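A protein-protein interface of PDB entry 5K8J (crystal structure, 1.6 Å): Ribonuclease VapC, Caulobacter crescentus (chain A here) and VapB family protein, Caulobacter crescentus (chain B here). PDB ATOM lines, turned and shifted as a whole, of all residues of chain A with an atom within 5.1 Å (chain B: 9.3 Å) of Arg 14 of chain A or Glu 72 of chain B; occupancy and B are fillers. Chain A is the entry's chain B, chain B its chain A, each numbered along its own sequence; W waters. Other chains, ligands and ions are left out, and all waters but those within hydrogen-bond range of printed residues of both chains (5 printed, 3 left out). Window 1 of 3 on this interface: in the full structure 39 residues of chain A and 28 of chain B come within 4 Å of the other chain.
The backbone carbonyl oxygen (O) of Met 65 of chain B sits at hydrogen-bond distance from the guanidinium group (NH1) of Arg 58 of chain A (3.5 Å).
NH2 of Arg 55 of chain A lies close to N of Glu 72 of chain B, 3.5 Å away.
The side-chain carboxylate (OE1) of Glu 40 of chain A lies within salt-bridge range of the guanidinium group (NE) of Arg 74 of chain B (2.8 Å).
The guanidinium group (NH1) of Arg 67 of chain B is in hydrogen-bond range of the backbone carbonyl oxygen (O) of Gly 16 of chain A (2.8 Å).
OE2 of Glu 72 of chain B is in salt-bridge range of NH1 of Arg 47 of chain A.
The backbone carbonyl oxygen of Leu 62 of chain B lies within hydrogen-bond range of the guanidinium group of Arg 58 of chain A, 2.8 Å away.
The guanidinium group of Arg 47 of chain A lies within hydrogen-bond range of the backbone carbonyl oxygen of Ile 73 of chain B, at 2.9 Å.
The side-chain carboxylate of Asp 15 of chain A is in hydrogen-bond range of the backbone NH of Glu 72 of chain B, 2.9 Å away.
NH1 of Arg 47 of chain A is in salt-bridge range of OD2 of Asp 75 of chain B (3.5 Å).
The guanidinium group (NH2) of Arg 14 of chain A lies within salt-bridge range of the side-chain carboxylate (OE1) of Glu 72 of chain B (2.7 Å).
O of Pro 66 of chain B lies within hydrogen-bond range of NH1 of Arg 58 of chain A, at 3.2 Å.
The guanidinium group (NH2) of Arg 55 of chain A lies within hydrogen-bond range of the backbone carbonyl oxygen (O) of Ser 70 of chain B (2.9 Å).
O of Arg 14 of chain A lies within hydrogen-bond range of NE of Arg 58 of chain A (2.7 Å).
The backbone NH (N) of Arg 14 of chain A sits close to the side-chain sulfur (SD) of Met 62 of chain A (3.6 Å).
The guanidinium group of Arg 55 of chain A is in salt-bridge range of the side-chain carboxylate of Asp 15 of chain A, at 3.2 Å.
The guanidinium group (NE) of Arg 14 of chain A lies within salt-bridge range of the side-chain carboxylate (OD1) of Asp 15 of chain A, 2.8 Å away.
The backbone carbonyl oxygen of Leu 13 of chain A lies within hydrogen-bond range of the guanidinium group of Arg 58 of chain A, at 3.4 Å.
O of Leu 41 of chain A lies within hydrogen-bond range of NH1 of Arg 14 of chain A (3.2 Å).
Among the printed residues, merely in contact across the chains: Gly 44 of chain A with Glu 72 of chain B, Asp 15 of chain A with Pro 68 of chain B, Asp 15 of chain A with Val 71 of chain B, His 12 of chain A with Val 71 of chain B, Ile 11 of chain A with Glu 72 of chain B, Asp 15 of chain A with Arg 67 of chain B, Asp 15 of chain A with Ser 70 of chain B, Glu 40 of chain A with Asp 75 of chain B, Arg 55 of chain A with Pro 68 of chain B, Ile 11 of chain A with Arg 74 of chain B, Leu 13 of chain A with Leu 62 of chain B, Met 62 of chain A with Leu 58 of chain B, Ile 11 of chain A with Val 71 of chain B and Arg 58 of chain A with Pro 68 of chain B.
Of chain B, only Glu 72 comes within 4 Å of Arg 14 of chain A.
Glu 72 of chain B touches just these residues of chain A: Ile 11 (3.7 Å), Arg 14 (2.7 Å), Asp 15 (2.9 Å), Gly 44 (3.4 Å), Arg 47 (2.9 Å) and Arg 55 (3.5 Å).
Ile 11 of chain A touches just these residues of chain B: Val 71 (3.9 Å), Glu 72 (3.7 Å) and Arg 74 (3.8 Å).
Leu 13 of chain A touches just one residue of chain B: Leu 62.
Asp 15 of chain A touches just these residues of chain B: Arg 67 (3.7 Å), Pro 68 (3.5 Å), Ser 70 (3.7 Å), Val 71 (3.5 Å) and Glu 72 (2.9 Å).
Of chain B, only Glu 72 (3.4 Å) comes within 4 Å of Gly 44 of chain A.
Of the printed residues of chain A, Ile 73 of chain B touches Arg 47 (2.9 Å).
Of the printed residues of chain A, Asp 75 of chain B touches Glu 40 (3.8 Å) and Arg 47 (3.5 Å).
Of the printed residues of chain A, Arg 67 of chain B touches Asp 15 (3.7 Å) and Gly 16 (2.8 Å).
Leu 59 of chain A touches none of the printed residues of chain B.
The nearest residue of chain B that does not touch Arg 14 of chain A is Pro 68 of chain B (4.2 Å).
The nearest residue of chain A that does not touch Glu 72 of chain B is Glu 40 of chain A (4.7 Å).
The nearest printed residue of chain A that does not touch Asp 75 of chain B is Ile 11 of chain A (6.1 Å).
Of the 16 printed residues of chain A, 12 touch a printed residue of chain B.
Hydrophobic or aromatic side chains of chain A within 4 Å of the printed part of chain B: Ile 11, His 12 and Leu 13.
Among the printed residues, 26 pairs touch across the chains.
Water W2 lies within hydrogen-bond range of OD1 of Asp 75 of chain B (2.5 Å), O of Ile 73 of chain B (2.7 Å) and NH2 of Arg 47 of chain A (2.9 Å).
Water W3 lies within hydrogen-bond range of O of Asp 75 of chain B (2.5 Å) and OE1 of Glu 40 of chain A (2.7 Å).
Water W1 lies within hydrogen-bond range of OD1 of Asn 63 of chain B (2.7 Å), NH2 of Arg 58 of chain A (3.0 Å) and O of Leu 62 of chain B (3.3 Å).
Water W4 lies within hydrogen-bond range of O of Gly 44 of chain A (2.7 Å), NH1 of Arg 55 of chain A (3.0 Å) and OE1 of Glu 72 of chain B (3.0 Å).
Water W5 lies within hydrogen-bond range of O of Glu 40 of chain A (2.8 Å), OE2 of Glu 72 of chain B (2.9 Å) and N of Gly 44 of chain A (3.2 Å).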
ATOM      1  N   ALA A  10      -5.326 -19.019 -24.134  1.00  0.00           N
ATOM      2  CA  ALA A  10      -5.846 -18.138 -23.100  1.00  0.00           C
ATOM      3  C   ALA A  10      -5.000 -18.191 -21.836  1.00  0.00           C
ATOM      4  O   ALA A  10      -4.840 -17.172 -21.156  1.00  0.00           O
ATOM      5  CB  ALA A  10      -7.293 -18.493 -22.791  1.00  0.00           C
ATOM      6  N   ILE A  11      -4.509 -19.373 -21.464  1.00  0.00           N
ATOM      7  CA  ILE A  11      -3.592 -19.479 -20.324  1.00  0.00           C
ATOM      8  C   ILE A  11      -2.345 -18.623 -20.543  1.00  0.00           C
ATOM      9  O   ILE A  11      -1.874 -17.927 -19.628  1.00  0.00           O
ATOM     10  CB  ILE A  11      -3.225 -20.954 -20.048  1.00  0.00           C
ATOM     11  CG1 ILE A  11      -4.386 -21.683 -19.409  1.00  0.00           C
ATOM     12  CG2 ILE A  11      -1.975 -21.061 -19.117  1.00  0.00           C
ATOM     13  CD1 ILE A  11      -4.214 -23.177 -19.334  1.00  0.00           C
ATOM     14  N   HIS A  12      -1.760 -18.685 -21.738  1.00  0.00           N
ATOM     15  CA  HIS A  12      -0.564 -17.899 -22.008  1.00  0.00           C
ATOM     16  C   HIS A  12      -0.852 -16.409 -21.945  1.00  0.00           C
ATOM     17  O   HIS A  12      -0.003 -15.621 -21.503  1.00  0.00           O
ATOM     18  CB  HIS A  12       0.003 -18.320 -23.367  1.00  0.00           C
ATOM     19  CG  HIS A  12       0.773 -19.611 -23.299  1.00  0.00           C
ATOM     20  ND1 HIS A  12       2.118 -19.685 -23.606  1.00  0.00           N
ATOM     21  CD2 HIS A  12       0.415 -20.850 -22.883  1.00  0.00           C
ATOM     22  CE1 HIS A  12       2.542 -20.922 -23.415  1.00  0.00           C
ATOM     23  NE2 HIS A  12       1.531 -21.649 -22.972  1.00  0.00           N
ATOM     24  N   LEU A  13      -2.059 -16.010 -22.329  1.00  0.00           N
ATOM     25  CA  LEU A  13      -2.482 -14.626 -22.160  1.00  0.00           C
ATOM     26  C   LEU A  13      -2.597 -14.275 -20.673  1.00  0.00           C
ATOM     27  O   LEU A  13      -1.980 -13.310 -20.198  1.00  0.00           O
ATOM     28  CB  LEU A  13      -3.806 -14.429 -22.919  1.00  0.00           C
ATOM     29  CG  LEU A  13      -4.399 -13.054 -23.176  1.00  0.00           C
ATOM     30  CD1 LEU A  13      -3.360 -12.130 -23.810  1.00  0.00           C
ATOM     31  CD2 LEU A  13      -5.600 -13.198 -24.088  1.00  0.00           C
ATOM     32  N   ARG A  14      -3.300 -15.103 -19.897  1.00  0.00           N
ATOM     33  CA  ARG A  14      -3.451 -14.851 -18.462  1.00  0.00           C
ATOM     34  C   ARG A  14      -2.101 -14.766 -17.754  1.00  0.00           C
ATOM     35  O   ARG A  14      -1.912 -13.939 -16.847  1.00  0.00           O
ATOM     36  CB  ARG A  14      -4.289 -15.951 -17.815  1.00  0.00           C
ATOM     37  CG  ARG A  14      -4.579 -15.685 -16.307  1.00  0.00           C
ATOM     38  CD  ARG A  14      -4.970 -16.944 -15.486  1.00  0.00           C
ATOM     39  NE  ARG A  14      -3.887 -17.931 -15.514  1.00  0.00           N
ATOM     40  CZ  ARG A  14      -4.046 -19.248 -15.440  1.00  0.00           C
ATOM     41  NH1 ARG A  14      -5.246 -19.791 -15.294  1.00  0.00           N
ATOM     42  NH2 ARG A  14      -2.986 -20.043 -15.521  1.00  0.00           N
ATOM     43  N   ASP A  15      -1.165 -15.640 -18.113  1.00  0.00           N
ATOM     44  CA  ASP A  15       0.099 -15.709 -17.399  1.00  0.00           C
ATOM     45  C   ASP A  15       1.194 -14.860 -18.030  1.00  0.00           C
ATOM     46  O   ASP A  15       2.316 -14.852 -17.509  1.00  0.00           O
ATOM     47  CB  ASP A  15       0.526 -17.168 -17.265  1.00  0.00           C
ATOM     48  CG  ASP A  15      -0.347 -17.915 -16.302  1.00  0.00           C
ATOM     49  OD1 ASP A  15      -1.131 -17.251 -15.571  1.00  0.00           O
ATOM     50  OD2 ASP A  15      -0.292 -19.158 -16.271  1.00  0.00           O
ATOM     51  N   GLY A  16       0.886 -14.078 -19.068  1.00  0.00           N
ATOM     52  CA  GLY A  16       1.770 -13.003 -19.479  1.00  0.00           C
ATOM     53  C   GLY A  16       2.821 -13.381 -20.496  1.00  0.00           C
ATOM     54  O   GLY A  16       3.913 -12.786 -20.506  1.00  0.00           O
ATOM     55  N   GLU A  40     -11.478 -23.963 -16.925  1.00  0.00           N
ATOM     56  CA  GLU A  40     -10.087 -24.353 -16.773  1.00  0.00           C
ATOM     57  C   GLU A  40      -9.257 -23.210 -16.214  1.00  0.00           C
ATOM     58  O   GLU A  40      -8.416 -23.433 -15.330  1.00  0.00           O
ATOM     59  CB  GLU A  40      -9.540 -24.849 -18.111  1.00  0.00           C
ATOM     60  CG  GLU A  40     -10.239 -26.075 -18.660  1.00  0.00           C
ATOM     61  CD  GLU A  40      -9.521 -26.571 -19.909  1.00  0.00           C
ATOM     62  OE1 GLU A  40      -8.455 -27.213 -19.724  1.00  0.00           O
ATOM     63  OE2 GLU A  40      -9.960 -26.222 -21.051  1.00  0.00           O
ATOM     64  N   LEU A  41      -9.492 -21.977 -16.696  1.00  0.00           N
ATOM     65  CA  LEU A  41      -8.747 -20.791 -16.237  1.00  0.00           C
ATOM     66  C   LEU A  41      -9.029 -20.491 -14.773  1.00  0.00           C
ATOM     67  O   LEU A  41      -8.117 -20.091 -14.022  1.00  0.00           O
ATOM     68  CB  LEU A  41      -9.116 -19.587 -17.105  1.00  0.00           C
ATOM     69  CG  LEU A  41      -8.554 -19.634 -18.522  1.00  0.00           C
ATOM     70  CD1 LEU A  41      -9.338 -18.756 -19.480  1.00  0.00           C
ATOM     71  CD2 LEU A  41      -7.085 -19.208 -18.513  1.00  0.00           C
ATOM     72  N   GLY A  44      -7.177 -22.941 -12.584  1.00  0.00           N
ATOM     73  CA  GLY A  44      -5.753 -22.661 -12.571  1.00  0.00           C
ATOM     74  C   GLY A  44      -5.349 -21.524 -11.646  1.00  0.00           C
ATOM     75  O   GLY A  44      -4.245 -21.524 -11.099  1.00  0.00           O
ATOM     76  N   VAL A  45      -6.236 -20.550 -11.441  1.00  0.00           N
ATOM     77  CA  VAL A  45      -5.931 -19.479 -10.500  1.00  0.00           C
ATOM     78  C   VAL A  45      -5.496 -20.056  -9.154  1.00  0.00           C
ATOM     79  O   VAL A  45      -4.579 -19.542  -8.519  1.00  0.00           O
ATOM     80  CB  VAL A  45      -7.151 -18.553 -10.331  1.00  0.00           C
ATOM     81  CG1 VAL A  45      -6.975 -17.596  -9.114  1.00  0.00           C
ATOM     82  CG2 VAL A  45      -7.395 -17.777 -11.584  1.00  0.00           C
ATOM     83  N   ARG A  47      -4.333 -23.156  -8.348  1.00  0.00           N
ATOM     84  CA  ARG A  47      -3.422 -24.304  -8.313  1.00  0.00           C
ATOM     85  C   ARG A  47      -2.157 -24.044  -7.529  1.00  0.00           C
ATOM     86  O   ARG A  47      -1.632 -24.972  -6.903  1.00  0.00           O
ATOM     87  CB  ARG A  47      -3.038 -24.729  -9.729  1.00  0.00           C
ATOM     88  CG  ARG A  47      -4.185 -25.432 -10.402  1.00  0.00           C
ATOM     89  CD  ARG A  47      -3.832 -25.956 -11.819  1.00  0.00           C
ATOM     90  NE  ARG A  47      -2.775 -26.944 -11.751  1.00  0.00           N
ATOM     91  CZ  ARG A  47      -2.112 -27.397 -12.808  1.00  0.00           C
ATOM     92  NH1 ARG A  47      -2.419 -26.947 -14.013  1.00  0.00           N
ATOM     93  NH2 ARG A  47      -1.149 -28.298 -12.669  1.00  0.00           N
ATOM     94  N   ARG A  55      -2.799 -14.233 -10.999  1.00  0.00           N
ATOM     95  CA  ARG A  55      -3.645 -14.944 -11.946  1.00  0.00           C
ATOM     96  C   ARG A  55      -5.098 -14.498 -11.827  1.00  0.00           C
ATOM     97  O   ARG A  55      -5.803 -14.371 -12.830  1.00  0.00           O
ATOM     98  CB  ARG A  55      -3.503 -16.452 -11.748  1.00  0.00           C
ATOM     99  CG  ARG A  55      -2.154 -16.967 -12.242  1.00  0.00           C
ATOM    100  CD  ARG A  55      -2.010 -18.479 -12.133  1.00  0.00           C
ATOM    101  NE  ARG A  55      -0.820 -18.888 -12.896  1.00  0.00           N
ATOM    102  CZ  ARG A  55       0.005 -19.879 -12.580  1.00  0.00           C
ATOM    103  NH1 ARG A  55      -0.183 -20.603 -11.491  1.00  0.00           N
ATOM    104  NH2 ARG A  55       1.038 -20.149 -13.377  1.00  0.00           N
ATOM    105  N   ARG A  58      -5.443 -10.832 -13.396  1.00  0.00           N
ATOM    106  CA  ARG A  58      -5.284 -10.827 -14.849  1.00  0.00           C
ATOM    107  C   ARG A  58      -6.424 -11.578 -15.523  1.00  0.00           C
ATOM    108  O   ARG A  58      -6.930 -11.137 -16.561  1.00  0.00           O
ATOM    109  CB  ARG A  58      -3.917 -11.412 -15.228  1.00  0.00           C
ATOM    110  CG  ARG A  58      -2.762 -10.523 -14.679  1.00  0.00           C
ATOM    111  CD  ARG A  58      -1.388 -11.141 -14.828  1.00  0.00           C
ATOM    112  NE  ARG A  58      -1.163 -11.387 -16.231  1.00  0.00           N
ATOM    113  CZ  ARG A  58      -0.596 -10.539 -17.075  1.00  0.00           C
ATOM    114  NH1 ARG A  58      -0.101  -9.373 -16.670  1.00  0.00           N
ATOM    115  NH2 ARG A  58      -0.517 -10.883 -18.348  1.00  0.00           N
ATOM    116  N   LEU A  59      -6.873 -12.690 -14.939  1.00  0.00           N
ATOM    117  CA  LEU A  59      -8.026 -13.366 -15.505  1.00  0.00           C
ATOM    118  C   LEU A  59      -9.255 -12.483 -15.417  1.00  0.00           C
ATOM    119  O   LEU A  59     -10.074 -12.458 -16.346  1.00  0.00           O
ATOM    120  CB  LEU A  59      -8.269 -14.709 -14.810  1.00  0.00           C
ATOM    121  CG  LEU A  59      -9.486 -15.517 -15.301  1.00  0.00           C
ATOM    122  CD1 LEU A  59      -9.407 -15.806 -16.798  1.00  0.00           C
ATOM    123  CD2 LEU A  59      -9.647 -16.842 -14.525  1.00  0.00           C
ATOM    124  N   MET A  62      -9.338 -10.133 -18.283  1.00  0.00           N
ATOM    125  CA  MET A  62      -9.709 -10.877 -19.492  1.00  0.00           C
ATOM    126  C   MET A  62     -11.187 -11.173 -19.565  1.00  0.00           C
ATOM    127  O   MET A  62     -11.816 -11.061 -20.622  1.00  0.00           O
ATOM    128  CB  MET A  62      -8.944 -12.194 -19.585  1.00  0.00           C
ATOM    129  CG  MET A  62      -7.451 -12.009 -19.656  1.00  0.00           C
ATOM    130  SD  MET A  62      -6.557 -13.707 -19.571  1.00  0.00           S
ATOM    131  CE  MET A  62      -7.379 -14.357 -21.173  1.00  0.00           C
ATOM    132  N   LEU B  58      -7.184  -4.374 -23.785  1.00  0.00           N
ATOM    133  CA  LEU B  58      -6.970  -5.521 -22.909  1.00  0.00           C
ATOM    134  C   LEU B  58      -5.485  -5.829 -22.800  1.00  0.00           C
ATOM    135  O   LEU B  58      -4.946  -5.980 -21.697  1.00  0.00           O
ATOM    136  CB  LEU B  58      -7.738  -6.737 -23.419  1.00  0.00           C
ATOM    137  CG  LEU B  58      -7.394  -8.081 -22.784  1.00  0.00           C
ATOM    138  CD1 LEU B  58      -7.641  -8.047 -21.284  1.00  0.00           C
ATOM    139  CD2 LEU B  58      -8.202  -9.197 -23.406  1.00  0.00           C
ATOM    140  N   LEU B  62      -3.121  -5.661 -19.455  1.00  0.00           N
ATOM    141  CA  LEU B  62      -2.318  -6.790 -18.991  1.00  0.00           C
ATOM    142  C   LEU B  62      -0.832  -6.435 -18.922  1.00  0.00           C
ATOM    143  O   LEU B  62      -0.134  -6.848 -17.990  1.00  0.00           O
ATOM    144  CB  LEU B  62      -2.542  -7.989 -19.906  1.00  0.00           C
ATOM    145  CG  LEU B  62      -3.937  -8.619 -19.810  1.00  0.00           C
ATOM    146  CD1 LEU B  62      -4.147  -9.647 -20.891  1.00  0.00           C
ATOM    147  CD2 LEU B  62      -4.170  -9.244 -18.436  1.00  0.00           C
ATOM    148  N   ASN B  63      -0.317  -5.707 -19.914  1.00  0.00           N
ATOM    149  CA  ASN B  63       1.111  -5.387 -19.916  1.00  0.00           C
ATOM    150  C   ASN B  63       1.494  -4.375 -18.847  1.00  0.00           C
ATOM    151  O   ASN B  63       2.669  -4.308 -18.469  1.00  0.00           O
ATOM    152  CB  ASN B  63       1.532  -4.889 -21.289  1.00  0.00           C
ATOM    153  CG  ASN B  63       1.592  -6.016 -22.316  1.00  0.00           C
ATOM    154  OD1 ASN B  63       1.685  -7.186 -21.953  1.00  0.00           O
ATOM    155  ND2 ASN B  63       1.554  -5.666 -23.593  1.00  0.00           N
ATOM    156  N   MET B  65       0.396  -4.669 -15.871  1.00  0.00           N
ATOM    157  CA  MET B  65       0.306  -5.433 -14.642  1.00  0.00           C
ATOM    158  C   MET B  65       1.477  -6.394 -14.536  1.00  0.00           C
ATOM    159  O   MET B  65       1.996  -6.836 -15.562  1.00  0.00           O
ATOM    160  CB  MET B  65      -0.997  -6.218 -14.614  1.00  0.00           C
ATOM    161  CG  MET B  65      -2.217  -5.343 -14.601  1.00  0.00           C
ATOM    162  SD  MET B  65      -3.789  -6.394 -15.046  1.00  0.00           S
ATOM    163  CE  MET B  65      -4.016  -7.327 -13.401  1.00  0.00           C
ATOM    164  N   PRO B  66       1.881  -6.736 -13.315  1.00  0.00           N
ATOM    165  CA  PRO B  66       2.876  -7.800 -13.149  1.00  0.00           C
ATOM    166  C   PRO B  66       2.312  -9.110 -13.668  1.00  0.00           C
ATOM    167  O   PRO B  66       1.101  -9.289 -13.747  1.00  0.00           O
ATOM    168  CB  PRO B  66       3.102  -7.856 -11.636  1.00  0.00           C
ATOM    169  CG  PRO B  66       2.520  -6.589 -11.098  1.00  0.00           C
ATOM    170  CD  PRO B  66       1.420  -6.215 -12.020  1.00  0.00           C
ATOM    171  N   ARG B  67       3.195 -10.041 -13.988  1.00  0.00           N
ATOM    172  CA  ARG B  67       2.748 -11.355 -14.407  1.00  0.00           C
ATOM    173  C   ARG B  67       3.215 -12.439 -13.446  1.00  0.00           C
ATOM    174  O   ARG B  67       4.182 -12.256 -12.692  1.00  0.00           O
ATOM    175  CB  ARG B  67       3.241 -11.672 -15.821  1.00  0.00           C
ATOM    176  CG  ARG B  67       4.699 -11.932 -15.916  1.00  0.00           C
ATOM    177  CD  ARG B  67       5.125 -12.028 -17.376  1.00  0.00           C
ATOM    178  NE  ARG B  67       6.567 -11.881 -17.514  1.00  0.00           N
ATOM    179  CZ  ARG B  67       7.236 -12.062 -18.648  1.00  0.00           C
ATOM    180  NH1 ARG B  67       6.591 -12.412 -19.755  1.00  0.00           N
ATOM    181  NH2 ARG B  67       8.555 -11.898 -18.674  1.00  0.00           N
ATOM    182  N   PRO B  68       2.521 -13.568 -13.419  1.00  0.00           N
ATOM    183  CA  PRO B  68       2.936 -14.687 -12.570  1.00  0.00           C
ATOM    184  C   PRO B  68       4.336 -15.150 -12.931  1.00  0.00           C
ATOM    185  O   PRO B  68       4.839 -14.882 -14.019  1.00  0.00           O
ATOM    186  CB  PRO B  68       1.905 -15.775 -12.885  1.00  0.00           C
ATOM    187  CG  PRO B  68       0.817 -15.091 -13.608  1.00  0.00           C
ATOM    188  CD  PRO B  68       1.390 -13.935 -14.291  1.00  0.00           C
ATOM    189  N   ASP B  69       4.953 -15.892 -12.003  1.00  0.00           N
ATOM    190  CA  ASP B  69       6.342 -16.316 -12.184  1.00  0.00           C
ATOM    191  C   ASP B  69       6.512 -17.322 -13.316  1.00  0.00           C
ATOM    192  O   ASP B  69       7.628 -17.478 -13.817  1.00  0.00           O
ATOM    193  CB  ASP B  69       6.881 -16.923 -10.890  1.00  0.00           C
ATOM    194  CG  ASP B  69       6.953 -15.909  -9.755  1.00  0.00           C
ATOM    195  OD1 ASP B  69       6.831 -16.319  -8.583  1.00  0.00           O
ATOM    196  OD2 ASP B  69       7.118 -14.705 -10.038  1.00  0.00           O
ATOM    197  N   SER B  70       5.446 -18.015 -13.717  1.00  0.00           N
ATOM    198  CA  SER B  70       5.548 -19.025 -14.764  1.00  0.00           C
ATOM    199  C   SER B  70       4.181 -19.209 -15.405  1.00  0.00           C
ATOM    200  O   SER B  70       3.161 -18.778 -14.860  1.00  0.00           O
ATOM    201  CB  SER B  70       6.046 -20.365 -14.217  1.00  0.00           C
ATOM    202  OG  SER B  70       5.038 -20.993 -13.449  1.00  0.00           O
ATOM    203  N   VAL B  71       4.179 -19.852 -16.572  1.00  0.00           N
ATOM    204  CA  VAL B  71       2.947 -20.145 -17.301  1.00  0.00           C
ATOM    205  C   VAL B  71       2.459 -21.524 -16.897  1.00  0.00           C
ATOM    206  O   VAL B  71       3.210 -22.504 -16.967  1.00  0.00           O
ATOM    207  CB  VAL B  71       3.171 -20.073 -18.819  1.00  0.00           C
ATOM    208  CG1 VAL B  71       1.893 -20.470 -19.585  1.00  0.00           C
ATOM    209  CG2 VAL B  71       3.650 -18.689 -19.231  1.00  0.00           C
ATOM    210  N   GLU B  72       1.188 -21.607 -16.502  1.00  0.00           N
ATOM    211  CA  GLU B  72       0.614 -22.865 -16.046  1.00  0.00           C
ATOM    212  C   GLU B  72       0.724 -23.934 -17.123  1.00  0.00           C
ATOM    213  O   GLU B  72       0.515 -23.667 -18.308  1.00  0.00           O
ATOM    214  CB  GLU B  72      -0.860 -22.666 -15.652  1.00  0.00           C
ATOM    215  CG  GLU B  72      -1.658 -23.979 -15.456  1.00  0.00           C
ATOM    216  CD  GLU B  72      -3.166 -23.769 -15.268  1.00  0.00           C
ATOM    217  OE1 GLU B  72      -3.610 -22.608 -15.234  1.00  0.00           O
ATOM    218  OE2 GLU B  72      -3.908 -24.778 -15.165  1.00  0.00           O
ATOM    219  N   ILE B  73       1.018 -25.162 -16.689  1.00  0.00           N
ATOM    220  CA  ILE B  73       0.975 -26.344 -17.540  1.00  0.00           C
ATOM    221  C   ILE B  73      -0.444 -26.897 -17.454  1.00  0.00           C
ATOM    222  O   ILE B  73      -0.865 -27.397 -16.410  1.00  0.00           O
ATOM    223  CB  ILE B  73       2.006 -27.384 -17.101  1.00  0.00           C
ATOM    224  CG1 ILE B  73       3.401 -26.757 -17.107  1.00  0.00           C
ATOM    225  CG2 ILE B  73       1.948 -28.602 -17.992  1.00  0.00           C
ATOM    226  CD1 ILE B  73       3.807 -26.175 -18.432  1.00  0.00           C
ATOM    227  N   ARG B  74      -1.180 -26.799 -18.548  1.00  0.00           N
ATOM    228  CA  ARG B  74      -2.591 -27.174 -18.555  1.00  0.00           C
ATOM    229  C   ARG B  74      -2.760 -28.668 -18.274  1.00  0.00           C
ATOM    230  O   ARG B  74      -1.967 -29.489 -18.743  1.00  0.00           O
ATOM    231  CB  ARG B  74      -3.189 -26.816 -19.912  1.00  0.00           C
ATOM    232  CG  ARG B  74      -4.629 -27.207 -20.070  1.00  0.00           C
ATOM    233  CD  ARG B  74      -5.061 -26.958 -21.468  1.00  0.00           C
ATOM    234  NE  ARG B  74      -6.479 -27.211 -21.679  1.00  0.00           N
ATOM    235  CZ  ARG B  74      -7.010 -27.446 -22.872  1.00  0.00           C
ATOM    236  NH1 ARG B  74      -6.240 -27.472 -23.943  1.00  0.00           N
ATOM    237  NH2 ARG B  74      -8.289 -27.651 -23.006  1.00  0.00           N
ATOM    238  N   ASP B  75      -3.920 -29.066 -17.762  1.00  0.00           N
ATOM    239  CA  ASP B  75      -4.352 -30.476 -17.865  1.00  0.00           C
ATOM    240  C   ASP B  75      -5.591 -30.578 -18.774  1.00  0.00           C
ATOM    241  O   ASP B  75      -6.682 -30.230 -18.328  1.00  0.00           O
ATOM    242  CB  ASP B  75      -4.675 -31.043 -16.468  1.00  0.00           C
ATOM    243  CG  ASP B  75      -4.024 -30.252 -15.298  1.00  0.00           C
ATOM    244  OD1 ASP B  75      -2.797 -30.390 -15.056  1.00  0.00           O
ATOM    245  OD2 ASP B  75      -4.763 -29.544 -14.563  1.00  0.00           O
ATOM    246  N   GLU B  76      -5.462 -31.073 -20.043  1.00  0.00           N
ATOM    247  CA  GLU B  76      -6.656 -31.171 -20.931  1.00  0.00           C
ATOM    248  C   GLU B  76      -7.482 -32.438 -20.701  1.00  0.00           C
ATOM    249  O   GLU B  76      -8.701 -32.470 -21.017  1.00  0.00           O
ATOM    250  CB  GLU B  76      -6.280 -31.124 -22.432  1.00  0.00           C
ATOM    251  CG  GLU B  76      -7.468 -30.980 -23.435  1.00  0.00           C
ATOM    252  CD  GLU B  76      -8.039 -32.325 -23.991  1.00  0.00           C
ATOM    253  OE1 GLU B  76      -9.128 -32.353 -24.646  1.00  0.00           O
ATOM    254  OE2 GLU B  76      -7.388 -33.364 -23.756  1.00  0.00           O
ATOM    255  N   LEU B  78      -9.345 -34.441 -18.612  1.00  0.00           N
ATOM    256  CA  LEU B  78     -10.197 -34.183 -17.463  1.00  0.00           C
ATOM    257  C   LEU B  78     -11.370 -35.152 -17.364  1.00  0.00           C
ATOM    258  O   LEU B  78     -11.921 -35.338 -16.264  1.00  0.00           O
ATOM    259  CB  LEU B  78     -10.731 -32.756 -17.534  1.00  0.00           C
ATOM    260  CG  LEU B  78      -9.676 -31.653 -17.476  1.00  0.00           C
ATOM    261  CD1 LEU B  78     -10.373 -30.287 -17.521  1.00  0.00           C
ATOM    262  CD2 LEU B  78      -8.842 -31.806 -16.223  1.00  0.00           C
HETATM  263  O   HOH W   1       1.093  -9.100 -20.102  1.00  0.00           O
HETATM  264  O   HOH W   2      -0.404 -29.676 -15.105  1.00  0.00           O
HETATM  265  O   HOH W   3      -7.506 -28.037 -17.346  1.00  0.00           O
HETATM  266  O   HOH W   4      -2.183 -22.586 -12.553  1.00  0.00           O
HETATM  267  O   HOH W   5      -6.674 -25.476 -14.507  1.00  0.00           O
